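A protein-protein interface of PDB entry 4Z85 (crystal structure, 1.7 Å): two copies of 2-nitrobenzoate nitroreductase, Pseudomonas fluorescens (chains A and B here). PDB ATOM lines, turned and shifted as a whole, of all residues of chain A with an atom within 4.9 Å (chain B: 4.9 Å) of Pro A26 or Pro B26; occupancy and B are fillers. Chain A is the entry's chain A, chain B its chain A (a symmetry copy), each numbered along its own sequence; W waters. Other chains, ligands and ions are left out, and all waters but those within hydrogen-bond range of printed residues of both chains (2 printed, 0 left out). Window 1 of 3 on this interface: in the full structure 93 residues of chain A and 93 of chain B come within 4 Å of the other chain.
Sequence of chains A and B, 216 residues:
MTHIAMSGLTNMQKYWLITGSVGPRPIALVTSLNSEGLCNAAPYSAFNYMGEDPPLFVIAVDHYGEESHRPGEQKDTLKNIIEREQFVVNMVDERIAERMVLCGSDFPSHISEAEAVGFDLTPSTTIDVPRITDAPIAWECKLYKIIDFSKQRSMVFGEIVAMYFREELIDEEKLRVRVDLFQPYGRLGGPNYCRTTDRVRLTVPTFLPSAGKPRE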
ATOM      1  N   VAL A  22      11.850 -33.930  11.023  1.00  0.00           N
ATOM      2  CA  VAL A  22      12.950 -32.968  10.909  1.00  0.00           C
ATOM      3  C   VAL A  22      13.899 -33.147  12.092  1.00  0.00           C
ATOM      4  O   VAL A  22      13.523 -32.984  13.245  1.00  0.00           O
ATOM      5  CB  VAL A  22      12.464 -31.480  10.819  1.00  0.00           C
ATOM      6  CG1 VAL A  22      11.486 -31.115  11.938  1.00  0.00           C
ATOM      7  CG2 VAL A  22      13.669 -30.531  10.850  1.00  0.00           C
ATOM      8  N   GLY A  23      15.137 -33.525  11.807  1.00  0.00           N
ATOM      9  CA  GLY A  23      16.072 -33.782  12.888  1.00  0.00           C
ATOM     10  C   GLY A  23      17.437 -34.110  12.326  1.00  0.00           C
ATOM     11  O   GLY A  23      17.593 -34.201  11.111  1.00  0.00           O
ATOM     12  N   PRO A  24      18.433 -34.252  13.198  1.00  0.00           N
ATOM     13  CA  PRO A  24      18.309 -33.931  14.618  1.00  0.00           C
ATOM     14  C   PRO A  24      18.235 -32.405  14.784  1.00  0.00           C
ATOM     15  O   PRO A  24      18.756 -31.682  13.924  1.00  0.00           O
ATOM     16  CB  PRO A  24      19.605 -34.502  15.202  1.00  0.00           C
ATOM     17  CG  PRO A  24      20.609 -34.278  14.075  1.00  0.00           C
ATOM     18  CD  PRO A  24      19.838 -34.478  12.797  1.00  0.00           C
ATOM     19  N   ARG A  25      17.561 -31.934  15.833  1.00  0.00           N
ATOM     20  CA  ARG A  25      17.370 -30.506  16.084  1.00  0.00           C
ATOM     21  C   ARG A  25      18.270 -30.019  17.216  1.00  0.00           C
ATOM     22  O   ARG A  25      18.467 -30.718  18.215  1.00  0.00           O
ATOM     23  CB  ARG A  25      15.905 -30.211  16.424  1.00  0.00           C
ATOM     24  CG  ARG A  25      14.939 -30.671  15.336  1.00  0.00           C
ATOM     25  CD  ARG A  25      13.524 -30.205  15.605  1.00  0.00           C
ATOM     26  NE  ARG A  25      12.901 -30.766  16.803  1.00  0.00           N
ATOM     27  CZ  ARG A  25      12.332 -31.968  16.881  1.00  0.00           C
ATOM     28  NH1 ARG A  25      12.389 -32.817  15.870  1.00  0.00           N
ATOM     29  NH2 ARG A  25      11.731 -32.336  18.015  1.00  0.00           N
ATOM     30  N   PRO A  26      18.822 -28.807  17.071  1.00  0.00           N
ATOM     31  CA  PRO A  26      19.605 -28.243  18.173  1.00  0.00           C
ATOM     32  C   PRO A  26      18.684 -27.798  19.302  1.00  0.00           C
ATOM     33  O   PRO A  26      17.518 -27.469  19.049  1.00  0.00           O
ATOM     34  CB  PRO A  26      20.280 -27.026  17.532  1.00  0.00           C
ATOM     35  CG  PRO A  26      19.259 -26.578  16.486  1.00  0.00           C
ATOM     36  CD  PRO A  26      18.651 -27.858  15.951  1.00  0.00           C
ATOM     37  N   ILE A  27      19.209 -27.781  20.518  1.00  0.00           N
ATOM     38  CA  ILE A  27      18.403 -27.486  21.709  1.00  0.00           C
ATOM     39  C   ILE A  27      18.869 -26.196  22.361  1.00  0.00           C
ATOM     40  O   ILE A  27      20.029 -26.061  22.750  1.00  0.00           O
ATOM     41  CB  ILE A  27      18.475 -28.625  22.725  1.00  0.00           C
ATOM     42  CG1 ILE A  27      18.041 -29.940  22.066  1.00  0.00           C
ATOM     43  CG2 ILE A  27      17.553 -28.337  23.924  1.00  0.00           C
ATOM     44  CD1 ILE A  27      18.318 -31.173  22.944  1.00  0.00           C
ATOM     45  N   ALA A  28      17.953 -25.244  22.459  1.00  0.00           N
ATOM     46  CA  ALA A  28      18.222 -24.002  23.177  1.00  0.00           C
ATOM     47  C   ALA A  28      17.650 -24.129  24.584  1.00  0.00           C
ATOM     48  O   ALA A  28      16.435 -24.125  24.755  1.00  0.00           O
ATOM     49  CB  ALA A  28      17.604 -22.802  22.447  1.00  0.00           C
ATOM     50  N   TYR A  44      14.038 -25.639  24.243  1.00  0.00           N
ATOM     51  CA  TYR A  44      13.281 -25.527  22.994  1.00  0.00           C
ATOM     52  C   TYR A  44      14.105 -26.055  21.835  1.00  0.00           C
ATOM     53  O   TYR A  44      15.245 -25.650  21.690  1.00  0.00           O
ATOM     54  CB  TYR A  44      12.925 -24.072  22.701  1.00  0.00           C
ATOM     55  CG  TYR A  44      12.106 -23.430  23.778  1.00  0.00           C
ATOM     56  CD1 TYR A  44      10.731 -23.561  23.783  1.00  0.00           C
ATOM     57  CD2 TYR A  44      12.715 -22.711  24.792  1.00  0.00           C
ATOM     58  CE1 TYR A  44       9.960 -22.982  24.783  1.00  0.00           C
ATOM     59  CE2 TYR A  44      11.958 -22.130  25.799  1.00  0.00           C
ATOM     60  CZ  TYR A  44      10.586 -22.273  25.781  1.00  0.00           C
ATOM     61  OH  TYR A  44       9.819 -21.696  26.768  1.00  0.00           O
ATOM     62  N   SER A  45      13.543 -26.926  21.004  1.00  0.00           N
ATOM     63  CA  SER A  45      14.289 -27.398  19.837  1.00  0.00           C
ATOM     64  C   SER A  45      13.677 -26.913  18.512  1.00  0.00           C
ATOM     65  O   SER A  45      14.170 -27.266  17.448  1.00  0.00           O
ATOM     66  CB  SER A  45      14.421 -28.940  19.855  1.00  0.00           C
ATOM     67  OG  SER A  45      13.192 -29.584  19.567  1.00  0.00           O
ATOM     68  N   PHE A  47      14.264 -24.284  16.813  1.00  0.00           N
ATOM     69  CA  PHE A  47      15.345 -23.331  17.091  1.00  0.00           C
ATOM     70  C   PHE A  47      16.389 -23.457  16.023  1.00  0.00           C
ATOM     71  O   PHE A  47      16.780 -24.579  15.690  1.00  0.00           O
ATOM     72  CB  PHE A  47      15.957 -23.643  18.470  1.00  0.00           C
ATOM     73  CG  PHE A  47      17.352 -23.079  18.718  1.00  0.00           C
ATOM     74  CD1 PHE A  47      17.624 -21.721  18.578  1.00  0.00           C
ATOM     75  CD2 PHE A  47      18.369 -23.918  19.162  1.00  0.00           C
ATOM     76  CE1 PHE A  47      18.900 -21.220  18.867  1.00  0.00           C
ATOM     77  CE2 PHE A  47      19.636 -23.433  19.459  1.00  0.00           C
ATOM     78  CZ  PHE A  47      19.897 -22.077  19.311  1.00  0.00           C
ATOM     79  N   ASN A  48      16.850 -22.325  15.485  1.00  0.00           N
ATOM     80  CA  ASN A  48      18.105 -22.358  14.737  1.00  0.00           C
ATOM     81  C   ASN A  48      18.627 -20.947  14.542  1.00  0.00           C
ATOM     82  O   ASN A  48      17.917 -19.986  14.786  1.00  0.00           O
ATOM     83  CB  ASN A  48      17.950 -23.051  13.371  1.00  0.00           C
ATOM     84  CG  ASN A  48      19.175 -23.888  13.004  1.00  0.00           C
ATOM     85  OD1 ASN A  48      20.294 -23.515  13.338  1.00  0.00           O
ATOM     86  ND2 ASN A  48      18.966 -25.033  12.344  1.00  0.00           N
ATOM     87  N   VAL B  22      26.002 -23.876  17.470  1.00  0.00           N
ATOM     88  CA  VAL B  22      24.630 -24.390  17.483  1.00  0.00           C
ATOM     89  C   VAL B  22      24.555 -25.650  16.623  1.00  0.00           C
ATOM     90  O   VAL B  22      24.817 -25.625  15.428  1.00  0.00           O
ATOM     91  CB  VAL B  22      23.570 -23.338  17.003  1.00  0.00           C
ATOM     92  CG1 VAL B  22      23.941 -22.704  15.660  1.00  0.00           C
ATOM     93  CG2 VAL B  22      22.186 -23.993  16.906  1.00  0.00           C
ATOM     94  N   GLY B  23      24.232 -26.773  17.245  1.00  0.00           N
ATOM     95  CA  GLY B  23      24.211 -28.021  16.501  1.00  0.00           C
ATOM     96  C   GLY B  23      23.730 -29.146  17.389  1.00  0.00           C
ATOM     97  O   GLY B  23      23.500 -28.934  18.577  1.00  0.00           O
ATOM     98  N   PRO B  24      23.542 -30.333  16.814  1.00  0.00           N
ATOM     99  CA  PRO B  24      23.600 -30.545  15.370  1.00  0.00           C
ATOM    100  C   PRO B  24      22.360 -29.911  14.720  1.00  0.00           C
ATOM    101  O   PRO B  24      21.326 -29.790  15.391  1.00  0.00           O
ATOM    102  CB  PRO B  24      23.580 -32.072  15.257  1.00  0.00           C
ATOM    103  CG  PRO B  24      22.691 -32.485  16.426  1.00  0.00           C
ATOM    104  CD  PRO B  24      22.986 -31.502  17.529  1.00  0.00           C
ATOM    105  N   ARG B  25      22.481 -29.472  13.467  1.00  0.00           N
ATOM    106  CA  ARG B  25      21.397 -28.804  12.746  1.00  0.00           C
ATOM    107  C   ARG B  25      20.766 -29.735  11.713  1.00  0.00           C
ATOM    108  O   ARG B  25      21.463 -30.504  11.044  1.00  0.00           O
ATOM    109  CB  ARG B  25      21.912 -27.537  12.055  1.00  0.00           C
ATOM    110  CG  ARG B  25      22.559 -26.554  13.026  1.00  0.00           C
ATOM    111  CD  ARG B  25      22.890 -25.237  12.358  1.00  0.00           C
ATOM    112  NE  ARG B  25      23.899 -25.310  11.302  1.00  0.00           N
ATOM    113  CZ  ARG B  25      25.216 -25.338  11.499  1.00  0.00           C
ATOM    114  NH1 ARG B  25      25.722 -25.414  12.718  1.00  0.00           N
ATOM    115  NH2 ARG B  25      26.037 -25.331  10.446  1.00  0.00           N
ATOM    116  N   PRO B  26      19.436 -29.667  11.572  1.00  0.00           N
ATOM    117  CA  PRO B  26      18.789 -30.455  10.519  1.00  0.00           C
ATOM    118  C   PRO B  26      19.067 -29.841   9.153  1.00  0.00           C
ATOM    119  O   PRO B  26      19.295 -28.629   9.061  1.00  0.00           O
ATOM    120  CB  PRO B  26      17.301 -30.334  10.860  1.00  0.00           C
ATOM    121  CG  PRO B  26      17.205 -28.947  11.495  1.00  0.00           C
ATOM    122  CD  PRO B  26      18.490 -28.779  12.280  1.00  0.00           C
ATOM    123  N   ILE B  27      19.035 -30.668   8.119  1.00  0.00           N
ATOM    124  CA  ILE B  27      19.396 -30.234   6.764  1.00  0.00           C
ATOM    125  C   ILE B  27      18.194 -30.312   5.841  1.00  0.00           C
ATOM    126  O   ILE B  27      17.597 -31.373   5.659  1.00  0.00           O
ATOM    127  CB  ILE B  27      20.533 -31.081   6.194  1.00  0.00           C
ATOM    128  CG1 ILE B  27      21.740 -31.038   7.138  1.00  0.00           C
ATOM    129  CG2 ILE B  27      20.958 -30.552   4.812  1.00  0.00           C
ATOM    130  CD1 ILE B  27      22.832 -32.056   6.765  1.00  0.00           C
ATOM    131  N   ALA B  28      17.836 -29.169   5.273  1.00  0.00           N
ATOM    132  CA  ALA B  28      16.781 -29.121   4.265  1.00  0.00           C
ATOM    133  C   ALA B  28      17.434 -29.126   2.888  1.00  0.00           C
ATOM    134  O   ALA B  28      18.045 -28.139   2.494  1.00  0.00           O
ATOM    135  CB  ALA B  28      15.909 -27.871   4.445  1.00  0.00           C
ATOM    136  N   TYR B  44      20.392 -26.541   2.988  1.00  0.00           N
ATOM    137  CA  TYR B  44      20.419 -25.453   3.968  1.00  0.00           C
ATOM    138  C   TYR B  44      20.254 -26.008   5.370  1.00  0.00           C
ATOM    139  O   TYR B  44      19.333 -26.773   5.595  1.00  0.00           O
ATOM    140  CB  TYR B  44      19.287 -24.461   3.712  1.00  0.00           C
ATOM    141  CG  TYR B  44      19.336 -23.838   2.351  1.00  0.00           C
ATOM    142  CD1 TYR B  44      20.108 -22.715   2.124  1.00  0.00           C
ATOM    143  CD2 TYR B  44      18.624 -24.387   1.298  1.00  0.00           C
ATOM    144  CE1 TYR B  44      20.173 -22.134   0.863  1.00  0.00           C
ATOM    145  CE2 TYR B  44      18.682 -23.819   0.034  1.00  0.00           C
ATOM    146  CZ  TYR B  44      19.458 -22.697  -0.168  1.00  0.00           C
ATOM    147  OH  TYR B  44      19.521 -22.116  -1.414  1.00  0.00           O
ATOM    148  N   SER B  45      21.110 -25.619   6.309  1.00  0.00           N
ATOM    149  CA  SER B  45      20.932 -26.083   7.685  1.00  0.00           C
ATOM    150  C   SER B  45      20.556 -24.942   8.646  1.00  0.00           C
ATOM    151  O   SER B  45      20.416 -25.173   9.841  1.00  0.00           O
ATOM    152  CB  SER B  45      22.193 -26.831   8.181  1.00  0.00           C
ATOM    153  OG  SER B  45      23.279 -25.950   8.416  1.00  0.00           O
ATOM    154  N   PHE B  47      17.696 -23.835   9.507  1.00  0.00           N
ATOM    155  CA  PHE B  47      16.415 -24.460   9.155  1.00  0.00           C
ATOM    156  C   PHE B  47      15.818 -25.069  10.388  1.00  0.00           C
ATOM    157  O   PHE B  47      16.528 -25.756  11.127  1.00  0.00           O
ATOM    158  CB  PHE B  47      16.654 -25.546   8.090  1.00  0.00           C
ATOM    159  CG  PHE B  47      15.550 -26.590   7.949  1.00  0.00           C
ATOM    160  CD1 PHE B  47      14.230 -26.225   7.702  1.00  0.00           C
ATOM    161  CD2 PHE B  47      15.867 -27.943   7.997  1.00  0.00           C
ATOM    162  CE1 PHE B  47      13.245 -27.204   7.521  1.00  0.00           C
ATOM    163  CE2 PHE B  47      14.902 -28.924   7.812  1.00  0.00           C
ATOM    164  CZ  PHE B  47      13.587 -28.548   7.571  1.00  0.00           C
ATOM    165  N   ASN B  48      14.524 -24.831  10.619  1.00  0.00           N
ATOM    166  CA  ASN B  48      13.808 -25.683  11.566  1.00  0.00           C
ATOM    167  C   ASN B  48      12.312 -25.493  11.402  1.00  0.00           C
ATOM    168  O   ASN B  48      11.875 -24.570  10.734  1.00  0.00           O
ATOM    169  CB  ASN B  48      14.213 -25.402  13.024  1.00  0.00           C
ATOM    170  CG  ASN B  48      14.272 -26.677  13.864  1.00  0.00           C
ATOM    171  OD1 ASN B  48      13.482 -27.589  13.652  1.00  0.00           O
ATOM    172  ND2 ASN B  48      15.227 -26.757  14.800  1.00  0.00           N
HETATM  173  O   HOH W   1      19.005 -33.519   8.943  1.00  0.00           O
HETATM  174  O   HOH W   2      21.823 -29.180  20.647  1.00  0.00           O
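The backbone carbonyl oxygen of Ser A45 is in hydrogen-bond range of the side-chain amide nitrogen of Asn B48. The side-chain amide nitrogen (ND2) of Asn B48 lies within hydrogen-bond range of the backbone carbonyl oxygen (O) of Phe A47 (2.8 Å). The side-chain amide nitrogen (ND2) of Asn A48 sits at hydrogen-bond distance from the backbone carbonyl oxygen (O) of Ser B45 (2.9 Å). O of Phe B47 is in hydrogen-bond range of ND2 of Asn A48, 2.8 Å away. The backbone carbonyl oxygen (O) of Pro A24 lies close to the backbone nitrogen (N) of Pro B26 (3.2 Å). O of Pro B24 lies close to N of Pro A26 (3.2 Å).
The backbone carbonyl oxygen (O) of Val A22 sits at hydrogen-bond distance from the guanidinium group (NH1) of Arg A25 (2.9 Å). The side-chain hydroxyl of Ser A45 sits at hydrogen-bond distance from the guanidinium group of Arg A25. O of Val B22 is in hydrogen-bond range of NH1 of Arg B25 (2.9 Å). OG of Ser B45 is in hydrogen-bond range of NE of Arg B25 (3.0 Å).
Val A22 touches Pro B26 (CG2 to CB, 3.6 Å). Val A22 touches Phe B47. CB of Pro B26 touches O of Gly A23, at 3.9 Å. O of Pro A24 touches O of Pro B24, 3.5 Å away. O of Pro B24 touches C of Arg A25, at 3.6 Å. OD1 of Asn B48 touches CD of Arg A25, 3.3 Å away. Val B22 touches Pro A26 (CG2 to CB, 3.6 Å). Pro A26 touches Pro B26 (CD to CD, 3.8 Å). CE2 of Phe A47 touches CG2 of Val B22, at 3.7 Å. Asn A48 touches Pro B26 (ND2 to CD, 3.8 Å).
Of the printed residues of chain B, Pro A24 touches Pro B24 (3.5 Å), Arg B25 (3.6 Å) and Pro B26 (3.2 Å). Pro A26 touches just these residues of chain B: Val B22 (3.6 Å), Gly B23 (3.9 Å), Pro B24 (3.2 Å), Pro B26 (3.8 Å) and Asn B48 (3.8 Å). Of the printed residues of chain A, Gly B23 touches Pro A26 (3.9 Å). Pro B26 touches just these residues of chain A: Val A22, Gly A23, Pro A24, Pro A26 and Asn A48. Ala B28 touches none of the printed residues of chain A. The nearest residue of chain B that does not touch Pro A26 is Arg B25 (4.3 Å). The nearest residue of chain A that does not touch Pro B26 is Arg A25 (4.3 Å). The nearest printed residue of chain A that does not touch Arg B25 is Pro A26 (4.3 Å).
Hydrophobic or aromatic side chains of chain B within 4 Å of the printed part of chain A: Val B22, Pro B24, Pro B26 and Phe B47. Along chain B the printed residues that touch a printed residue of chain A span positions 22 to 48. Among the printed residues, 20 pairs touch across the chains.
Pro A24 touches Pro B26, and with the chains exchanged Pro A26 touches Pro B24. Arg A25 touches Asn B48, and with the chains exchanged Asn A48 touches Arg B25. Pro B26 touches its own counterpart, Pro A26. Ser A45 touches Asn B48, and with the chains exchanged Asn A48 touches Ser B45. Of the 20 pairs that touch across the chains among the printed residues, 20 have their exchanged pair printed and touching as well.
Water W1 lies within hydrogen-bond range of the backbone carbonyl oxygen of Gly A23 and the backbone NH of Ile B27. Water W2 lies within hydrogen-bond range of O of Gly B23 and N of Ile A27.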
